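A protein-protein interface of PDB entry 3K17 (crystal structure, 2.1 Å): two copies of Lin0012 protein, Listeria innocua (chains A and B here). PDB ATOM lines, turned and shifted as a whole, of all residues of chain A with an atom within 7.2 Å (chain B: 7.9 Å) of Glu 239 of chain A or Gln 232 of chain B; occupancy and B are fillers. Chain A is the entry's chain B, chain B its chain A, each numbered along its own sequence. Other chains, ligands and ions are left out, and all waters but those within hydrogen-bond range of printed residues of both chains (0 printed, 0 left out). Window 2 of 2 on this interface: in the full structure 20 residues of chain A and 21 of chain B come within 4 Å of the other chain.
NZ of Lys 228 of chain B is in salt-bridge range of OE2 of Glu 239 of chain A.
Ser 231 of chain A touches Ala 235 of chain B, and with the chains exchanged Ala 235 of chain A touches Ser 231 of chain B. Ser 231 of chain A touches Gln 238 of chain B, and with the chains exchanged Gln 238 of chain A touches Ser 231 of chain B. Of the 7 pairs that touch across the chains among the printed residues, 4 have their exchanged pair printed and touching as well.
The backbone carbonyl oxygen of Gly 227 of chain B lies within hydrogen-bond range of the side-chain hydroxyl of Ser 231 of chain B (3.1 Å). O of Lys 228 of chain B is in hydrogen-bond range of OG of Ser 231 of chain B (2.9 Å). OE1 of Gln 232 of chain B sits close to O of Lys 228 of chain B (3.3 Å). A ring nitrogen (NE2) of His 234 of chain B lies within hydrogen-bond range of the side-chain amide oxygen (OE1) of Gln 238 of chain B (3.4 Å).
Among the printed residues, merely in contact across the chains: Gln 238 of chain A with Ser 231 of chain B (3.5 Å), Ser 231 of chain A with Gln 238 of chain B (3.6 Å), Ala 235 of chain A with Ser 231 of chain B (3.6 Å), Ser 231 of chain A with Ala 235 of chain B (3.7 Å), Glu 239 of chain A with Gln 232 of chain B (3.7 Å) and Gln 238 of chain A with Lys 228 of chain B (3.9 Å).
Printed residues of chain B within 4 Å of Glu 239 of chain A: Lys 228 and Gln 232. Of chain A, only Glu 239 comes within 4 Å of Gln 232 of chain B. Of the printed residues of chain A, Gln 238 of chain B touches Ser 231. Of the printed residues of chain A, Lys 228 of chain B touches Gln 238 (3.9 Å) and Glu 239 (2.9 Å). Printed residues of chain A within 4 Å of Ser 231 of chain B: Ala 235 (3.6 Å) and Gln 238 (3.5 Å). Of the printed residues of chain A, Ala 235 of chain B touches Ser 231 (3.7 Å). Of the printed residues of chain B, Gln 238 of chain A touches Lys 228 and Ser 231. Thr 226 of chain B touches none of the printed residues of chain A. Asn 291 of chain B touches none of the printed residues of chain A. The nearest residue of chain A that does not touch Gln 232 of chain B is Ala 235 of chain A (4.4 Å).
Of the 22 printed residues of chain B, 5 touch a printed residue of chain A. Hydrophobic or aromatic side chains of chain B within 4 Å of the printed part of chain A: Ala 235. Along chain B the printed residues that touch a printed residue of chain A span positions 228 to 238. Printed residues of chain A that touch a printed residue of chain B: Ser 231, Ala 235, Gln 238 and Glu 239. Among the printed residues, 7 pairs touch across the chains. Among the printed residues, Asp or Glu carboxylates within 4 Å of a Lys or Arg side-chain nitrogen of the other chain: Glu 239 of chain A with Lys 228 of chain B.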
ATOM      1  N   SER A 231     -12.493  10.355  -6.485  1.00  0.00           N
ATOM      2  CA  SER A 231     -12.075  11.587  -5.821  1.00  0.00           C
ATOM      3  C   SER A 231     -12.134  12.756  -6.797  1.00  0.00           C
ATOM      4  O   SER A 231     -12.514  13.866  -6.423  1.00  0.00           O
ATOM      5  CB  SER A 231     -10.654  11.443  -5.267  1.00  0.00           C
ATOM      6  OG  SER A 231      -9.721  11.189  -6.302  1.00  0.00           O
ATOM      7  N   ILE A 233     -14.148  13.109  -9.473  1.00  0.00           N
ATOM      8  CA  ILE A 233     -15.544  13.470  -9.686  1.00  0.00           C
ATOM      9  C   ILE A 233     -16.093  14.232  -8.493  1.00  0.00           C
ATOM     10  O   ILE A 233     -16.823  15.211  -8.652  1.00  0.00           O
ATOM     11  CB  ILE A 233     -16.423  12.223  -9.931  1.00  0.00           C
ATOM     12  CG1 ILE A 233     -15.974  11.520 -11.212  1.00  0.00           C
ATOM     13  CG2 ILE A 233     -17.891  12.630 -10.051  1.00  0.00           C
ATOM     14  CD1 ILE A 233     -16.069  12.386 -12.452  1.00  0.00           C
ATOM     15  N   HIS A 234     -15.740  13.782  -7.295  1.00  0.00           N
ATOM     16  CA  HIS A 234     -16.197  14.439  -6.081  1.00  0.00           C
ATOM     17  C   HIS A 234     -15.685  15.878  -6.080  1.00  0.00           C
ATOM     18  O   HIS A 234     -16.387  16.802  -5.671  1.00  0.00           O
ATOM     19  CB  HIS A 234     -15.673  13.702  -4.846  1.00  0.00           C
ATOM     20  CG  HIS A 234     -16.106  14.317  -3.553  1.00  0.00           C
ATOM     21  ND1 HIS A 234     -17.424  14.349  -3.149  1.00  0.00           N
ATOM     22  CD2 HIS A 234     -15.403  14.958  -2.589  1.00  0.00           C
ATOM     23  CE1 HIS A 234     -17.514  14.986  -1.994  1.00  0.00           C
ATOM     24  NE2 HIS A 234     -16.302  15.365  -1.633  1.00  0.00           N
ATOM     25  N   ALA A 235     -14.451  16.051  -6.540  1.00  0.00           N
ATOM     26  CA  ALA A 235     -13.838  17.371  -6.603  1.00  0.00           C
ATOM     27  C   ALA A 235     -14.553  18.201  -7.660  1.00  0.00           C
ATOM     28  O   ALA A 235     -14.791  19.393  -7.470  1.00  0.00           O
ATOM     29  CB  ALA A 235     -12.361  17.243  -6.949  1.00  0.00           C
ATOM     30  N   PHE A 236     -14.896  17.556  -8.773  1.00  0.00           N
ATOM     31  CA  PHE A 236     -15.588  18.222  -9.867  1.00  0.00           C
ATOM     32  C   PHE A 236     -16.928  18.766  -9.391  1.00  0.00           C
ATOM     33  O   PHE A 236     -17.323  19.874  -9.754  1.00  0.00           O
ATOM     34  CB  PHE A 236     -15.820  17.242 -11.015  1.00  0.00           C
ATOM     35  CG  PHE A 236     -16.618  17.816 -12.150  1.00  0.00           C
ATOM     36  CD1 PHE A 236     -16.069  18.788 -12.983  1.00  0.00           C
ATOM     37  CD2 PHE A 236     -17.913  17.378 -12.393  1.00  0.00           C
ATOM     38  CE1 PHE A 236     -16.794  19.312 -14.043  1.00  0.00           C
ATOM     39  CE2 PHE A 236     -18.651  17.896 -13.451  1.00  0.00           C
ATOM     40  CZ  PHE A 236     -18.089  18.867 -14.279  1.00  0.00           C
ATOM     41  N   LYS A 237     -17.627  17.982  -8.578  1.00  0.00           N
ATOM     42  CA  LYS A 237     -18.922  18.398  -8.057  1.00  0.00           C
ATOM     43  C   LYS A 237     -18.829  19.776  -7.403  1.00  0.00           C
ATOM     44  O   LYS A 237     -19.774  20.559  -7.447  1.00  0.00           O
ATOM     45  CB  LYS A 237     -19.440  17.377  -7.038  1.00  0.00           C
ATOM     46  CG  LYS A 237     -20.736  17.805  -6.351  1.00  0.00           C
ATOM     47  CD  LYS A 237     -21.217  16.802  -5.309  1.00  0.00           C
ATOM     48  CE  LYS A 237     -22.529  17.276  -4.676  1.00  0.00           C
ATOM     49  NZ  LYS A 237     -23.037  16.355  -3.615  1.00  0.00           N
ATOM     50  N   GLN A 238     -17.677  20.061  -6.806  1.00  0.00           N
ATOM     51  CA  GLN A 238     -17.439  21.327  -6.120  1.00  0.00           C
ATOM     52  C   GLN A 238     -17.030  22.432  -7.084  1.00  0.00           C
ATOM     53  O   GLN A 238     -17.598  23.520  -7.076  1.00  0.00           O
ATOM     54  CB  GLN A 238     -16.330  21.150  -5.079  1.00  0.00           C
ATOM     55  CG  GLN A 238     -16.499  19.930  -4.208  1.00  0.00           C
ATOM     56  CD  GLN A 238     -17.719  20.021  -3.329  1.00  0.00           C
ATOM     57  OE1 GLN A 238     -18.311  19.006  -2.970  1.00  0.00           O
ATOM     58  NE2 GLN A 238     -18.095  21.240  -2.964  1.00  0.00           N
ATOM     59  N   GLU A 239     -16.036  22.134  -7.910  1.00  0.00           N
ATOM     60  CA  GLU A 239     -15.495  23.074  -8.880  1.00  0.00           C
ATOM     61  C   GLU A 239     -16.473  23.517  -9.972  1.00  0.00           C
ATOM     62  O   GLU A 239     -16.435  24.669 -10.404  1.00  0.00           O
ATOM     63  CB  GLU A 239     -14.244  22.461  -9.521  1.00  0.00           C
ATOM     64  CG  GLU A 239     -13.561  23.316 -10.584  1.00  0.00           C
ATOM     65  CD  GLU A 239     -12.827  24.522 -10.011  1.00  0.00           C
ATOM     66  OE1 GLU A 239     -12.145  25.227 -10.791  1.00  0.00           O
ATOM     67  OE2 GLU A 239     -12.931  24.769  -8.789  1.00  0.00           O
ATOM     68  N   ASP A 240     -17.351  22.615 -10.411  1.00  0.00           N
ATOM     69  CA  ASP A 240     -18.305  22.927 -11.476  1.00  0.00           C
ATOM     70  C   ASP A 240     -19.727  22.439 -11.176  1.00  0.00           C
ATOM     71  O   ASP A 240     -20.222  21.499 -11.798  1.00  0.00           O
ATOM     72  CB  ASP A 240     -17.820  22.299 -12.783  1.00  0.00           C
ATOM     73  CG  ASP A 240     -18.564  22.821 -13.992  1.00  0.00           C
ATOM     74  OD1 ASP A 240     -19.661  23.400 -13.820  1.00  0.00           O
ATOM     75  OD2 ASP A 240     -18.054  22.638 -15.119  1.00  0.00           O
ATOM     76  N   SER A 241     -20.385  23.104 -10.234  1.00  0.00           N
ATOM     77  CA  SER A 241     -21.735  22.746  -9.823  1.00  0.00           C
ATOM     78  C   SER A 241     -22.788  22.708 -10.933  1.00  0.00           C
ATOM     79  O   SER A 241     -23.672  21.844 -10.933  1.00  0.00           O
ATOM     80  CB  SER A 241     -22.209  23.706  -8.727  1.00  0.00           C
ATOM     81  OG  SER A 241     -23.557  23.439  -8.380  1.00  0.00           O
ATOM     82  N   LYS A 242     -22.719  23.649 -11.865  1.00  0.00           N
ATOM     83  CA  LYS A 242     -23.706  23.678 -12.933  1.00  0.00           C
ATOM     84  C   LYS A 242     -23.671  22.422 -13.802  1.00  0.00           C
ATOM     85  O   LYS A 242     -24.715  21.830 -14.102  1.00  0.00           O
ATOM     86  CB  LYS A 242     -23.510  24.908 -13.820  1.00  0.00           C
ATOM     87  CG  LYS A 242     -24.557  25.008 -14.914  1.00  0.00           C
ATOM     88  CD  LYS A 242     -24.352  26.230 -15.789  1.00  0.00           C
ATOM     89  CE  LYS A 242     -25.438  26.306 -16.859  1.00  0.00           C
ATOM     90  NZ  LYS A 242     -25.285  27.519 -17.703  1.00  0.00           N
ATOM     91  N   TYR B  21      -3.377  21.200   6.348  1.00  0.00           N
ATOM     92  CA  TYR B  21      -3.524  20.198   5.299  1.00  0.00           C
ATOM     93  C   TYR B  21      -2.939  18.868   5.731  1.00  0.00           C
ATOM     94  O   TYR B  21      -3.634  17.856   5.724  1.00  0.00           O
ATOM     95  CB  TYR B  21      -2.896  20.684   3.987  1.00  0.00           C
ATOM     96  CG  TYR B  21      -3.795  21.651   3.242  1.00  0.00           C
ATOM     97  CD1 TYR B  21      -4.912  21.193   2.538  1.00  0.00           C
ATOM     98  CD2 TYR B  21      -3.563  23.027   3.282  1.00  0.00           C
ATOM     99  CE1 TYR B  21      -5.777  22.076   1.898  1.00  0.00           C
ATOM    100  CE2 TYR B  21      -4.423  23.923   2.644  1.00  0.00           C
ATOM    101  CZ  TYR B  21      -5.527  23.441   1.955  1.00  0.00           C
ATOM    102  OH  TYR B  21      -6.392  24.318   1.330  1.00  0.00           O
ATOM    103  N   SER B 225     -14.587  28.904   0.136  1.00  0.00           N
ATOM    104  CA  SER B 225     -15.478  27.757   0.056  1.00  0.00           C
ATOM    105  C   SER B 225     -14.531  26.576   0.230  1.00  0.00           C
ATOM    106  O   SER B 225     -14.141  25.925  -0.738  1.00  0.00           O
ATOM    107  CB  SER B 225     -16.162  27.705  -1.314  1.00  0.00           C
ATOM    108  OG  SER B 225     -15.209  27.751  -2.364  1.00  0.00           O
ATOM    109  N   THR B 226     -14.143  26.337   1.478  1.00  0.00           N
ATOM    110  CA  THR B 226     -13.217  25.266   1.834  1.00  0.00           C
ATOM    111  C   THR B 226     -13.397  23.987   1.031  1.00  0.00           C
ATOM    112  O   THR B 226     -12.429  23.433   0.508  1.00  0.00           O
ATOM    113  CB  THR B 226     -13.341  24.912   3.323  1.00  0.00           C
ATOM    114  OG1 THR B 226     -13.140  26.092   4.108  1.00  0.00           O
ATOM    115  CG2 THR B 226     -12.302  23.868   3.711  1.00  0.00           C
ATOM    116  N   GLY B 227     -14.640  23.520   0.950  1.00  0.00           N
ATOM    117  CA  GLY B 227     -14.937  22.297   0.228  1.00  0.00           C
ATOM    118  C   GLY B 227     -14.125  22.128  -1.035  1.00  0.00           C
ATOM    119  O   GLY B 227     -13.399  21.144  -1.191  1.00  0.00           O
ATOM    120  N   LYS B 228     -14.237  23.099  -1.934  1.00  0.00           N
ATOM    121  CA  LYS B 228     -13.526  23.058  -3.202  1.00  0.00           C
ATOM    122  C   LYS B 228     -12.029  22.775  -3.038  1.00  0.00           C
ATOM    123  O   LYS B 228     -11.478  21.916  -3.725  1.00  0.00           O
ATOM    124  CB  LYS B 228     -13.718  24.376  -3.948  1.00  0.00           C
ATOM    125  CG  LYS B 228     -13.555  24.255  -5.450  1.00  0.00           C
ATOM    126  CD  LYS B 228     -13.369  25.614  -6.098  1.00  0.00           C
ATOM    127  CE  LYS B 228     -12.005  26.201  -5.747  1.00  0.00           C
ATOM    128  NZ  LYS B 228     -11.782  27.532  -6.376  1.00  0.00           N
ATOM    129  N   LEU B 229     -11.377  23.496  -2.129  1.00  0.00           N
ATOM    130  CA  LEU B 229      -9.946  23.315  -1.896  1.00  0.00           C
ATOM    131  C   LEU B 229      -9.597  21.967  -1.284  1.00  0.00           C
ATOM    132  O   LEU B 229      -8.673  21.296  -1.736  1.00  0.00           O
ATOM    133  CB  LEU B 229      -9.396  24.433  -1.005  1.00  0.00           C
ATOM    134  CG  LEU B 229      -9.158  25.779  -1.694  1.00  0.00           C
ATOM    135  CD1 LEU B 229     -10.484  26.373  -2.152  1.00  0.00           C
ATOM    136  CD2 LEU B 229      -8.453  26.724  -0.733  1.00  0.00           C
ATOM    137  N   VAL B 230     -10.332  21.571  -0.253  1.00  0.00           N
ATOM    138  CA  VAL B 230     -10.081  20.295   0.396  1.00  0.00           C
ATOM    139  C   VAL B 230     -10.281  19.131  -0.572  1.00  0.00           C
ATOM    140  O   VAL B 230      -9.453  18.223  -0.638  1.00  0.00           O
ATOM    141  CB  VAL B 230     -11.005  20.099   1.615  1.00  0.00           C
ATOM    142  CG1 VAL B 230     -10.780  18.731   2.229  1.00  0.00           C
ATOM    143  CG2 VAL B 230     -10.730  21.178   2.643  1.00  0.00           C
ATOM    144  N   SER B 231     -11.377  19.158  -1.326  1.00  0.00           N
ATOM    145  CA  SER B 231     -11.660  18.089  -2.275  1.00  0.00           C
ATOM    146  C   SER B 231     -10.569  18.017  -3.342  1.00  0.00           C
ATOM    147  O   SER B 231     -10.175  16.929  -3.764  1.00  0.00           O
ATOM    148  CB  SER B 231     -13.025  18.302  -2.936  1.00  0.00           C
ATOM    149  OG  SER B 231     -13.031  19.453  -3.759  1.00  0.00           O
ATOM    150  N   GLN B 232     -10.077  19.173  -3.773  1.00  0.00           N
ATOM    151  CA  GLN B 232      -9.029  19.205  -4.783  1.00  0.00           C
ATOM    152  C   GLN B 232      -7.755  18.556  -4.241  1.00  0.00           C
ATOM    153  O   GLN B 232      -7.115  17.763  -4.934  1.00  0.00           O
ATOM    154  CB  GLN B 232      -8.743  20.648  -5.216  1.00  0.00           C
ATOM    155  CG  GLN B 232      -9.903  21.312  -5.950  1.00  0.00           C
ATOM    156  CD  GLN B 232      -9.627  22.763  -6.315  1.00  0.00           C
ATOM    157  OE1 GLN B 232      -9.265  23.576  -5.460  1.00  0.00           O
ATOM    158  NE2 GLN B 232      -9.804  23.097  -7.589  1.00  0.00           N
ATOM    159  N   ILE B 233      -7.399  18.885  -3.000  1.00  0.00           N
ATOM    160  CA  ILE B 233      -6.200  18.329  -2.382  1.00  0.00           C
ATOM    161  C   ILE B 233      -6.327  16.822  -2.155  1.00  0.00           C
ATOM    162  O   ILE B 233      -5.386  16.071  -2.404  1.00  0.00           O
ATOM    163  CB  ILE B 233      -5.881  19.020  -1.030  1.00  0.00           C
ATOM    164  CG1 ILE B 233      -5.560  20.499  -1.259  1.00  0.00           C
ATOM    165  CG2 ILE B 233      -4.683  18.344  -0.363  1.00  0.00           C
ATOM    166  CD1 ILE B 233      -4.352  20.733  -2.148  1.00  0.00           C
ATOM    167  N   HIS B 234      -7.487  16.377  -1.686  1.00  0.00           N
ATOM    168  CA  HIS B 234      -7.688  14.954  -1.450  1.00  0.00           C
ATOM    169  C   HIS B 234      -7.507  14.191  -2.759  1.00  0.00           C
ATOM    170  O   HIS B 234      -6.922  13.107  -2.783  1.00  0.00           O
ATOM    171  CB  HIS B 234      -9.085  14.686  -0.901  1.00  0.00           C
ATOM    172  CG  HIS B 234      -9.339  13.243  -0.595  1.00  0.00           C
ATOM    173  ND1 HIS B 234      -8.736  12.589   0.457  1.00  0.00           N
ATOM    174  CD2 HIS B 234     -10.100  12.318  -1.227  1.00  0.00           C
ATOM    175  CE1 HIS B 234      -9.115  11.323   0.461  1.00  0.00           C
ATOM    176  NE2 HIS B 234      -9.942  11.132  -0.550  1.00  0.00           N
ATOM    177  N   ALA B 235      -8.013  14.763  -3.845  1.00  0.00           N
ATOM    178  CA  ALA B 235      -7.894  14.136  -5.154  1.00  0.00           C
ATOM    179  C   ALA B 235      -6.431  14.138  -5.574  1.00  0.00           C
ATOM    180  O   ALA B 235      -5.942  13.168  -6.152  1.00  0.00           O
ATOM    181  CB  ALA B 235      -8.734  14.883  -6.176  1.00  0.00           C
ATOM    182  N   PHE B 236      -5.738  15.235  -5.283  1.00  0.00           N
ATOM    183  CA  PHE B 236      -4.326  15.346  -5.617  1.00  0.00           C
ATOM    184  C   PHE B 236      -3.577  14.205  -4.940  1.00  0.00           C
ATOM    185  O   PHE B 236      -2.669  13.609  -5.515  1.00  0.00           O
ATOM    186  CB  PHE B 236      -3.765  16.681  -5.130  1.00  0.00           C
ATOM    187  CG  PHE B 236      -2.274  16.790  -5.268  1.00  0.00           C
ATOM    188  CD1 PHE B 236      -1.680  16.832  -6.526  1.00  0.00           C
ATOM    189  CD2 PHE B 236      -1.461  16.819  -4.141  1.00  0.00           C
ATOM    190  CE1 PHE B 236      -0.296  16.899  -6.662  1.00  0.00           C
ATOM    191  CE2 PHE B 236      -0.073  16.887  -4.265  1.00  0.00           C
ATOM    192  CZ  PHE B 236       0.510  16.926  -5.528  1.00  0.00           C
ATOM    193  N   LYS B 237      -3.966  13.915  -3.704  1.00  0.00           N
ATOM    194  CA  LYS B 237      -3.358  12.844  -2.930  1.00  0.00           C
ATOM    195  C   LYS B 237      -3.451  11.508  -3.677  1.00  0.00           C
ATOM    196  O   LYS B 237      -2.545  10.680  -3.601  1.00  0.00           O
ATOM    197  CB  LYS B 237      -4.058  12.738  -1.574  1.00  0.00           C
ATOM    198  CG  LYS B 237      -3.581  11.597  -0.696  1.00  0.00           C
ATOM    199  CD  LYS B 237      -4.336  11.575   0.627  1.00  0.00           C
ATOM    200  CE  LYS B 237      -3.917  10.389   1.480  1.00  0.00           C
ATOM    201  NZ  LYS B 237      -4.650  10.348   2.778  1.00  0.00           N
ATOM    202  N   GLN B 238      -4.547  11.313  -4.403  1.00  0.00           N
ATOM    203  CA  GLN B 238      -4.770  10.082  -5.158  1.00  0.00           C
ATOM    204  C   GLN B 238      -4.117  10.159  -6.537  1.00  0.00           C
ATOM    205  O   GLN B 238      -3.672   9.155  -7.085  1.00  0.00           O
ATOM    206  CB  GLN B 238      -6.269   9.844  -5.332  1.00  0.00           C
ATOM    207  CG  GLN B 238      -7.097  10.119  -4.086  1.00  0.00           C
ATOM    208  CD  GLN B 238      -6.825   9.141  -2.959  1.00  0.00           C
ATOM    209  OE1 GLN B 238      -7.327   9.308  -1.847  1.00  0.00           O
ATOM    210  NE2 GLN B 238      -6.036   8.111  -3.243  1.00  0.00           N
ATOM    211  N   GLU B 239      -4.071  11.368  -7.085  1.00  0.00           N
ATOM    212  CA  GLU B 239      -3.499  11.629  -8.402  1.00  0.00           C
ATOM    213  C   GLU B 239      -1.974  11.763  -8.376  1.00  0.00           C
ATOM    214  O   GLU B 239      -1.328  11.743  -9.422  1.00  0.00           O
ATOM    215  CB  GLU B 239      -4.130  12.910  -8.971  1.00  0.00           C
ATOM    216  CG  GLU B 239      -3.423  13.537 -10.169  1.00  0.00           C
ATOM    217  CD  GLU B 239      -3.620  12.761 -11.457  1.00  0.00           C
ATOM    218  OE1 GLU B 239      -3.161  11.600 -11.540  1.00  0.00           O
ATOM    219  OE2 GLU B 239      -4.238  13.317 -12.392  1.00  0.00           O
ATOM    220  N   LEU B 284       2.601  22.747  -2.722  1.00  0.00           N
ATOM    221  CA  LEU B 284       1.416  21.902  -2.763  1.00  0.00           C
ATOM    222  C   LEU B 284       0.354  22.545  -3.643  1.00  0.00           C
ATOM    223  O   LEU B 284      -0.249  21.883  -4.488  1.00  0.00           O
ATOM    224  CB  LEU B 284       0.863  21.691  -1.345  1.00  0.00           C
ATOM    225  CG  LEU B 284      -0.470  20.941  -1.238  1.00  0.00           C
ATOM    226  CD1 LEU B 284      -0.345  19.579  -1.894  1.00  0.00           C
ATOM    227  CD2 LEU B 284      -0.869  20.792   0.225  1.00  0.00           C
ATOM    228  N   ALA B 288      -0.814  20.672  -7.069  1.00  0.00           N
ATOM    229  CA  ALA B 288      -2.203  20.226  -7.101  1.00  0.00           C
ATOM    230  C   ALA B 288      -3.105  21.132  -7.931  1.00  0.00           C
ATOM    231  O   ALA B 288      -4.257  20.789  -8.207  1.00  0.00           O
ATOM    232  CB  ALA B 288      -2.746  20.126  -5.676  1.00  0.00           C
ATOM    233  N   GLY B 289      -2.584  22.286  -8.332  1.00  0.00           N
ATOM    234  CA  GLY B 289      -3.391  23.210  -9.102  1.00  0.00           C
ATOM    235  C   GLY B 289      -4.430  23.839  -8.193  1.00  0.00           C
ATOM    236  O   GLY B 289      -5.564  24.085  -8.600  1.00  0.00           O
ATOM    237  N   VAL B 290      -4.041  24.085  -6.947  1.00  0.00           N
ATOM    238  CA  VAL B 290      -4.930  24.688  -5.963  1.00  0.00           C
ATOM    239  C   VAL B 290      -4.359  26.024  -5.518  1.00  0.00           C
ATOM    240  O   VAL B 290      -3.216  26.104  -5.062  1.00  0.00           O
ATOM    241  CB  VAL B 290      -5.094  23.791  -4.724  1.00  0.00           C
ATOM    242  CG1 VAL B 290      -6.005  24.470  -3.711  1.00  0.00           C
ATOM    243  CG2 VAL B 290      -5.664  22.438  -5.135  1.00  0.00           C
ATOM    244  N   ASN B 291      -5.165  27.070  -5.647  1.00  0.00           N
ATOM    245  CA  ASN B 291      -4.740  28.410  -5.277  1.00  0.00           C
ATOM    246  C   ASN B 291      -4.766  28.638  -3.766  1.00  0.00           C
ATOM    247  O   ASN B 291      -5.614  29.374  -3.255  1.00  0.00           O
ATOM    248  CB  ASN B 291      -5.626  29.435  -5.990  1.00  0.00           C
ATOM    249  CG  ASN B 291      -5.238  30.862  -5.672  1.00  0.00           C
ATOM    250  OD1 ASN B 291      -4.055  31.195  -5.606  1.00  0.00           O
ATOM    251  ND2 ASN B 291      -6.237  31.720  -5.487  1.00  0.00           N
ATOM    252  N   ILE B 292      -3.838  28.001  -3.052  1.00  0.00           N
ATOM    253  CA  ILE B 292      -3.765  28.151  -1.601  1.00  0.00           C
ATOM    254  C   ILE B 292      -3.307  29.562  -1.259  1.00  0.00           C
ATOM    255  O   ILE B 292      -3.999  30.301  -0.559  1.00  0.00           O
ATOM    256  CB  ILE B 292      -2.788  27.137  -0.972  1.00  0.00           C
ATOM    257  CG1 ILE B 292      -3.278  25.712  -1.242  1.00  0.00           C
ATOM    258  CG2 ILE B 292      -2.673  27.389   0.526  1.00  0.00           C
ATOM    259  CD1 ILE B 292      -2.358  24.635  -0.718  1.00  0.00           C
